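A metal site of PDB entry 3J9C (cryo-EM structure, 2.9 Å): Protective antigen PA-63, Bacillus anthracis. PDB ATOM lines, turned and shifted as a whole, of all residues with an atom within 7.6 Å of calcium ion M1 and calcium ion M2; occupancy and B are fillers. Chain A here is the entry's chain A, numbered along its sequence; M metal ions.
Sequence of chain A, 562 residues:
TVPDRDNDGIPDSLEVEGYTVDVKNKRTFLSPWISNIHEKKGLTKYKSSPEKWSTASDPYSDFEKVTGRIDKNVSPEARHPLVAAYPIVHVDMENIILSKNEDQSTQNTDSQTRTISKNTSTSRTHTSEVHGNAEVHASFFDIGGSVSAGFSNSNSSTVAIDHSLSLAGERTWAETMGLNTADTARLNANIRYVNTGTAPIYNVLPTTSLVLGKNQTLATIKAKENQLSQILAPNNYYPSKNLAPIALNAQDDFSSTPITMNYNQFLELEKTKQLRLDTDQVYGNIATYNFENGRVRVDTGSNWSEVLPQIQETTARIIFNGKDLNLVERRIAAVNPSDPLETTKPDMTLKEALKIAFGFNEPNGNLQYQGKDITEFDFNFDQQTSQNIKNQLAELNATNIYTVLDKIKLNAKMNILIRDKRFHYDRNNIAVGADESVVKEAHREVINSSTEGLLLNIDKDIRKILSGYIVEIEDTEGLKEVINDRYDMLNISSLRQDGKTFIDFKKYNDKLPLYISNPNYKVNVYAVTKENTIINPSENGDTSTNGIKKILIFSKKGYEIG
Of the 26 residues printed, 6 come within 4 Å of calcium ion M1.
OD1 of Asp 12 touches calcium ion M2, 3.8 Å away.
Pro 50 touches calcium ion M2 (O to CA, 3.7 Å).
Seven residues have an atom within 4 Å of calcium ion M2: Asp 4, Asp 6, Asp 8, Ile 10, Asp 12, Glu 15 and Pro 50.
The nearest printed residue that does not touch calcium ion M2 is Pro 11 (4.5 Å).
Calcium ion M1 is bound by OD2 of Asp 6 (2.3 Å).
Calcium ion M1 is bound by OD2 of Asp 62.
Calcium ion M1 is bound by O of Lys 52, at 2.4 Å.
Calcium ion M1 is bound by O of Ser 49 (2.5 Å).
Calcium ion M1 is bound by OE1 of Glu 15 (2.7 Å).
Calcium ion M1 is bound by OD2 of Asp 8, at 2.7 Å.
The side-chain carboxylate (OE2) of Glu 15 binds calcium ion M1, 2.8 Å away.
Calcium ion M1 has seven donor atoms within binding distance.
The backbone NH of Asp 62 is in hydrogen-bond range of the backbone carbonyl oxygen of Trp 53 (3.4 Å).
The backbone NH (N) of Asp 4 lies within hydrogen-bond range of the side-chain carboxylate (OD2) of Asp 12 (3.4 Å).
OD2 of Asp 4 is in hydrogen-bond range of N of Gly 9 (2.9 Å).
The backbone carbonyl oxygen (O) of Thr 55 sits at hydrogen-bond distance from the side-chain amino group (NZ) of Lys 52 (3.2 Å).
The backbone NH of Ser 49 sits at hydrogen-bond distance from the side-chain hydroxyl of Thr 55, at 2.9 Å.
The backbone NH (N) of Glu 51 sits close to the side-chain hydroxyl (OG) of Ser 49 (3.4 Å).
OD1 of Asp 12 is in hydrogen-bond range of N of Arg 5 (3.0 Å).
N of Asp 12 is in hydrogen-bond range of O of Pro 3 (3.3 Å).
Calcium ion M2 is bound by O of Ile 10 (2.3 Å), OD1 of Asp 4 (2.4 Å), OD1 of Asp 6 (2.4 Å), OE2 of Glu 15 (2.4 Å) and OD1 of Asp 8 (2.5 Å).
Calcium ion M2 has five donor atoms within binding distance.
Slightly farther from calcium ion M2 lies the side-chain carboxylate (OD2) of Asp 6 (3.1 Å).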
ATOM      1  N   PRO A   3     -35.286  12.676  17.108  1.00  0.00           N
ATOM      2  CA  PRO A   3     -35.346  13.512  18.321  1.00  0.00           C
ATOM      3  C   PRO A   3     -34.048  14.255  18.646  1.00  0.00           C
ATOM      4  O   PRO A   3     -32.960  13.718  18.432  1.00  0.00           O
ATOM      5  CB  PRO A   3     -35.675  12.499  19.416  1.00  0.00           C
ATOM      6  CG  PRO A   3     -36.372  11.402  18.723  1.00  0.00           C
ATOM      7  CD  PRO A   3     -35.726  11.293  17.379  1.00  0.00           C
ATOM      8  N   ASP A   4     -34.176  15.464  19.182  1.00  0.00           N
ATOM      9  CA  ASP A   4     -33.017  16.279  19.557  1.00  0.00           C
ATOM     10  C   ASP A   4     -33.402  17.340  20.602  1.00  0.00           C
ATOM     11  O   ASP A   4     -33.619  18.502  20.248  1.00  0.00           O
ATOM     12  CB  ASP A   4     -32.406  16.941  18.326  1.00  0.00           C
ATOM     13  CG  ASP A   4     -31.056  17.556  18.599  1.00  0.00           C
ATOM     14  OD1 ASP A   4     -30.482  17.306  19.683  1.00  0.00           O
ATOM     15  OD2 ASP A   4     -30.557  18.313  17.730  1.00  0.00           O
ATOM     16  N   ARG A   5     -33.511  16.927  21.854  1.00  0.00           N
ATOM     17  CA  ARG A   5     -34.060  17.767  22.914  1.00  0.00           C
ATOM     18  C   ARG A   5     -33.254  19.023  23.240  1.00  0.00           C
ATOM     19  O   ARG A   5     -33.833  20.062  23.564  1.00  0.00           O
ATOM     20  CB  ARG A   5     -34.242  16.935  24.190  1.00  0.00           C
ATOM     21  CG  ARG A   5     -35.138  15.718  23.997  1.00  0.00           C
ATOM     22  CD  ARG A   5     -34.790  14.600  24.977  1.00  0.00           C
ATOM     23  NE  ARG A   5     -35.535  14.686  26.229  1.00  0.00           N
ATOM     24  CZ  ARG A   5     -36.465  13.813  26.605  1.00  0.00           C
ATOM     25  NH1 ARG A   5     -36.764  12.779  25.828  1.00  0.00           N
ATOM     26  NH2 ARG A   5     -37.091  13.963  27.765  1.00  0.00           N
ATOM     27  N   ASP A   6     -31.927  18.944  23.152  1.00  0.00           N
ATOM     28  CA  ASP A   6     -31.092  20.097  23.506  1.00  0.00           C
ATOM     29  C   ASP A   6     -30.819  21.010  22.319  1.00  0.00           C
ATOM     30  O   ASP A   6     -30.174  22.050  22.464  1.00  0.00           O
ATOM     31  CB  ASP A   6     -29.757  19.647  24.108  1.00  0.00           C
ATOM     32  CG  ASP A   6     -28.883  18.886  23.123  1.00  0.00           C
ATOM     33  OD1 ASP A   6     -29.190  18.861  21.910  1.00  0.00           O
ATOM     34  OD2 ASP A   6     -27.883  18.304  23.582  1.00  0.00           O
ATOM     35  N   ASN A   7     -31.281  20.587  21.149  1.00  0.00           N
ATOM     36  CA  ASN A   7     -31.226  21.376  19.928  1.00  0.00           C
ATOM     37  C   ASN A   7     -29.815  21.617  19.385  1.00  0.00           C
ATOM     38  O   ASN A   7     -29.598  22.534  18.601  1.00  0.00           O
ATOM     39  CB  ASN A   7     -31.919  22.727  20.153  1.00  0.00           C
ATOM     40  CG  ASN A   7     -32.629  23.246  18.930  1.00  0.00           C
ATOM     41  OD1 ASN A   7     -32.973  22.474  18.026  1.00  0.00           O
ATOM     42  ND2 ASN A   7     -32.869  24.544  18.896  1.00  0.00           N
ATOM     43  N   ASP A   8     -28.846  20.800  19.807  1.00  0.00           N
ATOM     44  CA  ASP A   8     -27.451  21.015  19.423  1.00  0.00           C
ATOM     45  C   ASP A   8     -27.029  20.368  18.098  1.00  0.00           C
ATOM     46  O   ASP A   8     -25.926  20.600  17.618  1.00  0.00           O
ATOM     47  CB  ASP A   8     -26.501  20.542  20.521  1.00  0.00           C
ATOM     48  CG  ASP A   8     -26.472  19.029  20.669  1.00  0.00           C
ATOM     49  OD1 ASP A   8     -27.293  18.325  20.038  1.00  0.00           O
ATOM     50  OD2 ASP A   8     -25.598  18.548  21.419  1.00  0.00           O
ATOM     51  N   GLY A   9     -27.912  19.555  17.521  1.00  0.00           N
ATOM     52  CA  GLY A   9     -27.617  18.894  16.256  1.00  0.00           C
ATOM     53  C   GLY A   9     -27.186  17.440  16.342  1.00  0.00           C
ATOM     54  O   GLY A   9     -27.148  16.752  15.328  1.00  0.00           O
ATOM     55  N   ILE A  10     -26.845  16.981  17.539  1.00  0.00           N
ATOM     56  CA  ILE A  10     -26.605  15.556  17.756  1.00  0.00           C
ATOM     57  C   ILE A  10     -27.851  14.895  18.322  1.00  0.00           C
ATOM     58  O   ILE A  10     -28.340  15.293  19.383  1.00  0.00           O
ATOM     59  CB  ILE A  10     -25.431  15.306  18.712  1.00  0.00           C
ATOM     60  CG1 ILE A  10     -24.231  16.158  18.319  1.00  0.00           C
ATOM     61  CG2 ILE A  10     -25.062  13.822  18.709  1.00  0.00           C
ATOM     62  CD1 ILE A  10     -22.997  15.908  19.157  1.00  0.00           C
ATOM     63  N   PRO A  11     -28.383  13.870  17.633  1.00  0.00           N
ATOM     64  CA  PRO A  11     -29.599  13.174  18.079  1.00  0.00           C
ATOM     65  C   PRO A  11     -29.415  12.515  19.445  1.00  0.00           C
ATOM     66  O   PRO A  11     -28.325  12.031  19.744  1.00  0.00           O
ATOM     67  CB  PRO A  11     -29.809  12.114  16.987  1.00  0.00           C
ATOM     68  CG  PRO A  11     -29.098  12.660  15.791  1.00  0.00           C
ATOM     69  CD  PRO A  11     -27.906  13.380  16.328  1.00  0.00           C
ATOM     70  N   ASP A  12     -30.477  12.498  20.246  1.00  0.00           N
ATOM     71  CA  ASP A  12     -30.392  12.106  21.654  1.00  0.00           C
ATOM     72  C   ASP A  12     -29.821  10.713  21.873  1.00  0.00           C
ATOM     73  O   ASP A  12     -28.924  10.506  22.705  1.00  0.00           O
ATOM     74  CB  ASP A  12     -31.788  12.175  22.286  1.00  0.00           C
ATOM     75  CG  ASP A  12     -32.451  13.527  22.095  1.00  0.00           C
ATOM     76  OD1 ASP A  12     -31.730  14.550  22.140  1.00  0.00           O
ATOM     77  OD2 ASP A  12     -33.680  13.565  21.897  1.00  0.00           O
ATOM     78  N   SER A  13     -30.330   9.743  21.104  1.00  0.00           N
ATOM     79  CA  SER A  13     -29.892   8.363  21.233  1.00  0.00           C
ATOM     80  C   SER A  13     -28.415   8.232  20.887  1.00  0.00           C
ATOM     81  O   SER A  13     -27.702   7.415  21.481  1.00  0.00           O
ATOM     82  CB  SER A  13     -30.735   7.466  20.334  1.00  0.00           C
ATOM     83  OG  SER A  13     -30.771   7.969  19.011  1.00  0.00           O
ATOM     84  N   GLU A  15     -26.243  10.625  21.428  1.00  0.00           N
ATOM     85  CA  GLU A  15     -25.545  11.239  22.545  1.00  0.00           C
ATOM     86  C   GLU A  15     -25.413  10.307  23.720  1.00  0.00           C
ATOM     87  O   GLU A  15     -24.386  10.309  24.406  1.00  0.00           O
ATOM     88  CB  GLU A  15     -26.269  12.508  22.998  1.00  0.00           C
ATOM     89  CG  GLU A  15     -26.262  13.606  21.971  1.00  0.00           C
ATOM     90  CD  GLU A  15     -26.105  14.967  22.605  1.00  0.00           C
ATOM     91  OE1 GLU A  15     -25.501  15.041  23.695  1.00  0.00           O
ATOM     92  OE2 GLU A  15     -26.587  15.951  22.014  1.00  0.00           O
ATOM     93  N   TYR A  19     -21.162   7.943  20.009  1.00  0.00           N
ATOM     94  CA  TYR A  19     -21.099   8.350  18.615  1.00  0.00           C
ATOM     95  C   TYR A  19     -19.698   8.810  18.245  1.00  0.00           C
ATOM     96  O   TYR A  19     -18.802   8.824  19.088  1.00  0.00           O
ATOM     97  CB  TYR A  19     -22.099   9.470  18.329  1.00  0.00           C
ATOM     98  CG  TYR A  19     -21.818  10.741  19.100  1.00  0.00           C
ATOM     99  CD1 TYR A  19     -22.308  10.917  20.383  1.00  0.00           C
ATOM    100  CD2 TYR A  19     -21.073  11.758  18.536  1.00  0.00           C
ATOM    101  CE1 TYR A  19     -22.054  12.062  21.099  1.00  0.00           C
ATOM    102  CE2 TYR A  19     -20.809  12.920  19.239  1.00  0.00           C
ATOM    103  CZ  TYR A  19     -21.306  13.072  20.520  1.00  0.00           C
ATOM    104  OH  TYR A  19     -21.064  14.222  21.224  1.00  0.00           O
ATOM    105  N   LYS A  47     -19.580  10.470  24.255  1.00  0.00           N
ATOM    106  CA  LYS A  47     -20.874  10.492  24.915  1.00  0.00           C
ATOM    107  C   LYS A  47     -21.080  11.895  25.454  1.00  0.00           C
ATOM    108  O   LYS A  47     -20.119  12.574  25.805  1.00  0.00           O
ATOM    109  CB  LYS A  47     -20.950   9.452  26.044  1.00  0.00           C
ATOM    110  CG  LYS A  47     -20.911   7.998  25.582  1.00  0.00           C
ATOM    111  CD  LYS A  47     -20.833   7.058  26.777  1.00  0.00           C
ATOM    112  CE  LYS A  47     -20.949   5.590  26.370  1.00  0.00           C
ATOM    113  NZ  LYS A  47     -22.357   5.105  26.407  1.00  0.00           N
ATOM    114  N   SER A  48     -22.325  12.328  25.506  1.00  0.00           N
ATOM    115  CA  SER A  48     -22.634  13.675  25.981  1.00  0.00           C
ATOM    116  C   SER A  48     -24.044  13.691  26.532  1.00  0.00           C
ATOM    117  O   SER A  48     -24.755  12.701  26.473  1.00  0.00           O
ATOM    118  CB  SER A  48     -22.474  14.702  24.861  1.00  0.00           C
ATOM    119  OG  SER A  48     -22.975  14.223  23.627  1.00  0.00           O
ATOM    120  N   SER A  49     -24.454  14.844  27.074  1.00  0.00           N
ATOM    121  CA  SER A  49     -25.794  14.940  27.638  1.00  0.00           C
ATOM    122  C   SER A  49     -26.790  15.305  26.550  1.00  0.00           C
ATOM    123  O   SER A  49     -26.679  16.371  25.948  1.00  0.00           O
ATOM    124  CB  SER A  49     -25.829  15.963  28.766  1.00  0.00           C
ATOM    125  OG  SER A  49     -27.174  16.328  29.039  1.00  0.00           O
ATOM    126  N   PRO A  50     -27.776  14.428  26.315  1.00  0.00           N
ATOM    127  CA  PRO A  50     -28.800  14.644  25.287  1.00  0.00           C
ATOM    128  C   PRO A  50     -29.573  15.920  25.546  1.00  0.00           C
ATOM    129  O   PRO A  50     -30.061  16.534  24.598  1.00  0.00           O
ATOM    130  CB  PRO A  50     -29.701  13.422  25.419  1.00  0.00           C
ATOM    131  CG  PRO A  50     -29.480  12.940  26.825  1.00  0.00           C
ATOM    132  CD  PRO A  50     -28.044  13.230  27.126  1.00  0.00           C
ATOM    133  N   GLU A  51     -29.720  16.275  26.815  1.00  0.00           N
ATOM    134  CA  GLU A  51     -30.521  17.420  27.215  1.00  0.00           C
ATOM    135  C   GLU A  51     -29.760  18.733  27.402  1.00  0.00           C
ATOM    136  O   GLU A  51     -30.365  19.770  27.638  1.00  0.00           O
ATOM    137  CB  GLU A  51     -31.276  17.080  28.499  1.00  0.00           C
ATOM    138  CG  GLU A  51     -32.539  16.256  28.251  1.00  0.00           C
ATOM    139  CD  GLU A  51     -33.372  16.060  29.498  1.00  0.00           C
ATOM    140  OE1 GLU A  51     -32.814  16.184  30.607  1.00  0.00           O
ATOM    141  OE2 GLU A  51     -34.590  15.781  29.375  1.00  0.00           O
ATOM    142  N   LYS A  52     -28.430  18.693  27.302  1.00  0.00           N
ATOM    143  CA  LYS A  52     -27.625  19.911  27.406  1.00  0.00           C
ATOM    144  C   LYS A  52     -26.964  20.261  26.086  1.00  0.00           C
ATOM    145  O   LYS A  52     -26.227  19.468  25.513  1.00  0.00           O
ATOM    146  CB  LYS A  52     -26.545  19.780  28.482  1.00  0.00           C
ATOM    147  CG  LYS A  52     -27.104  19.544  29.877  1.00  0.00           C
ATOM    148  CD  LYS A  52     -25.996  19.536  30.926  1.00  0.00           C
ATOM    149  CE  LYS A  52     -25.306  20.882  30.999  1.00  0.00           C
ATOM    150  NZ  LYS A  52     -24.333  20.926  32.121  1.00  0.00           N
ATOM    151  N   TRP A  53     -27.200  21.488  25.614  1.00  0.00           N
ATOM    152  CA  TRP A  53     -26.683  21.956  24.334  1.00  0.00           C
ATOM    153  C   TRP A  53     -25.160  21.998  24.355  1.00  0.00           C
ATOM    154  O   TRP A  53     -24.507  21.870  23.319  1.00  0.00           O
ATOM    155  CB  TRP A  53     -27.251  23.335  24.025  1.00  0.00           C
ATOM    156  CG  TRP A  53     -26.762  23.961  22.749  1.00  0.00           C
ATOM    157  CD1 TRP A  53     -27.318  23.849  21.518  1.00  0.00           C
ATOM    158  CD2 TRP A  53     -25.631  24.822  22.605  1.00  0.00           C
ATOM    159  NE1 TRP A  53     -26.602  24.579  20.605  1.00  0.00           N
ATOM    160  CE2 TRP A  53     -25.561  25.191  21.249  1.00  0.00           C
ATOM    161  CE3 TRP A  53     -24.668  25.320  23.496  1.00  0.00           C
ATOM    162  CZ2 TRP A  53     -24.557  26.033  20.752  1.00  0.00           C
ATOM    163  CZ3 TRP A  53     -23.672  26.151  23.003  1.00  0.00           C
ATOM    164  CH2 TRP A  53     -23.622  26.497  21.641  1.00  0.00           C
ATOM    165  N   SER A  54     -24.611  22.177  25.553  1.00  0.00           N
ATOM    166  CA  SER A  54     -23.204  21.896  25.822  1.00  0.00           C
ATOM    167  C   SER A  54     -23.098  21.142  27.141  1.00  0.00           C
ATOM    168  O   SER A  54     -23.538  21.640  28.177  1.00  0.00           O
ATOM    169  CB  SER A  54     -22.380  23.172  25.869  1.00  0.00           C
ATOM    170  OG  SER A  54     -21.162  22.937  26.561  1.00  0.00           O
ATOM    171  N   THR A  55     -22.511  19.950  27.105  1.00  0.00           N
ATOM    172  CA  THR A  55     -22.466  19.104  28.288  1.00  0.00           C
ATOM    173  C   THR A  55     -21.592  19.699  29.382  1.00  0.00           C
ATOM    174  O   THR A  55     -21.879  19.558  30.569  1.00  0.00           O
ATOM    175  CB  THR A  55     -21.951  17.693  27.934  1.00  0.00           C
ATOM    176  OG1 THR A  55     -22.752  17.145  26.870  1.00  0.00           O
ATOM    177  CG2 THR A  55     -22.031  16.769  29.130  1.00  0.00           C
ATOM    178  N   SER A  61     -21.185  24.076  21.657  1.00  0.00           N
ATOM    179  CA  SER A  61     -22.062  22.917  21.595  1.00  0.00           C
ATOM    180  C   SER A  61     -21.259  21.654  21.361  1.00  0.00           C
ATOM    181  O   SER A  61     -20.175  21.703  20.783  1.00  0.00           O
ATOM    182  CB  SER A  61     -23.116  23.057  20.494  1.00  0.00           C
ATOM    183  OG  SER A  61     -22.626  22.629  19.239  1.00  0.00           O
ATOM    184  N   ASP A  62     -21.797  20.523  21.818  1.00  0.00           N
ATOM    185  CA  ASP A  62     -21.101  19.251  21.698  1.00  0.00           C
ATOM    186  C   ASP A  62     -20.828  18.954  20.230  1.00  0.00           C
ATOM    187  O   ASP A  62     -19.773  18.405  19.886  1.00  0.00           O
ATOM    188  CB  ASP A  62     -21.933  18.151  22.337  1.00  0.00           C
ATOM    189  CG  ASP A  62     -22.339  18.481  23.751  1.00  0.00           C
ATOM    190  OD1 ASP A  62     -21.624  19.272  24.411  1.00  0.00           O
ATOM    191  OD2 ASP A  62     -23.385  17.968  24.219  1.00  0.00           O
ATOM    192  N   PHE A  63     -21.761  19.352  19.373  1.00  0.00           N
ATOM    193  CA  PHE A  63     -21.594  19.189  17.938  1.00  0.00           C
ATOM    194  C   PHE A  63     -20.442  20.042  17.418  1.00  0.00           C
ATOM    195  O   PHE A  63     -19.565  19.549  16.696  1.00  0.00           O
ATOM    196  CB  PHE A  63     -22.883  19.561  17.207  1.00  0.00           C
ATOM    197  CG  PHE A  63     -22.807  19.402  15.721  1.00  0.00           C
ATOM    198  CD1 PHE A  63     -22.851  18.142  15.145  1.00  0.00           C
ATOM    199  CD2 PHE A  63     -22.681  20.510  14.900  1.00  0.00           C
ATOM    200  CE1 PHE A  63     -22.775  17.993  13.771  1.00  0.00           C
ATOM    201  CE2 PHE A  63     -22.612  20.367  13.528  1.00  0.00           C
ATOM    202  CZ  PHE A  63     -22.659  19.102  12.960  1.00  0.00           C
ATOM    203  N   PRO A  81     -16.310  16.771  24.292  1.00  0.00           N
ATOM    204  CA  PRO A  81     -17.514  17.359  24.888  1.00  0.00           C
ATOM    205  C   PRO A  81     -17.526  17.375  26.409  1.00  0.00           C
ATOM    206  O   PRO A  81     -18.143  18.260  27.000  1.00  0.00           O
ATOM    207  CB  PRO A  81     -18.637  16.464  24.357  1.00  0.00           C
ATOM    208  CG  PRO A  81     -18.109  15.898  23.124  1.00  0.00           C
ATOM    209  CD  PRO A  81     -16.641  15.692  23.342  1.00  0.00           C
HETATM  210 CA    CA M   1     -25.699  17.679  23.992  1.00  0.00          CA
HETATM  211 CA    CA M   2     -28.749  16.655  21.161  1.00  0.00          CA
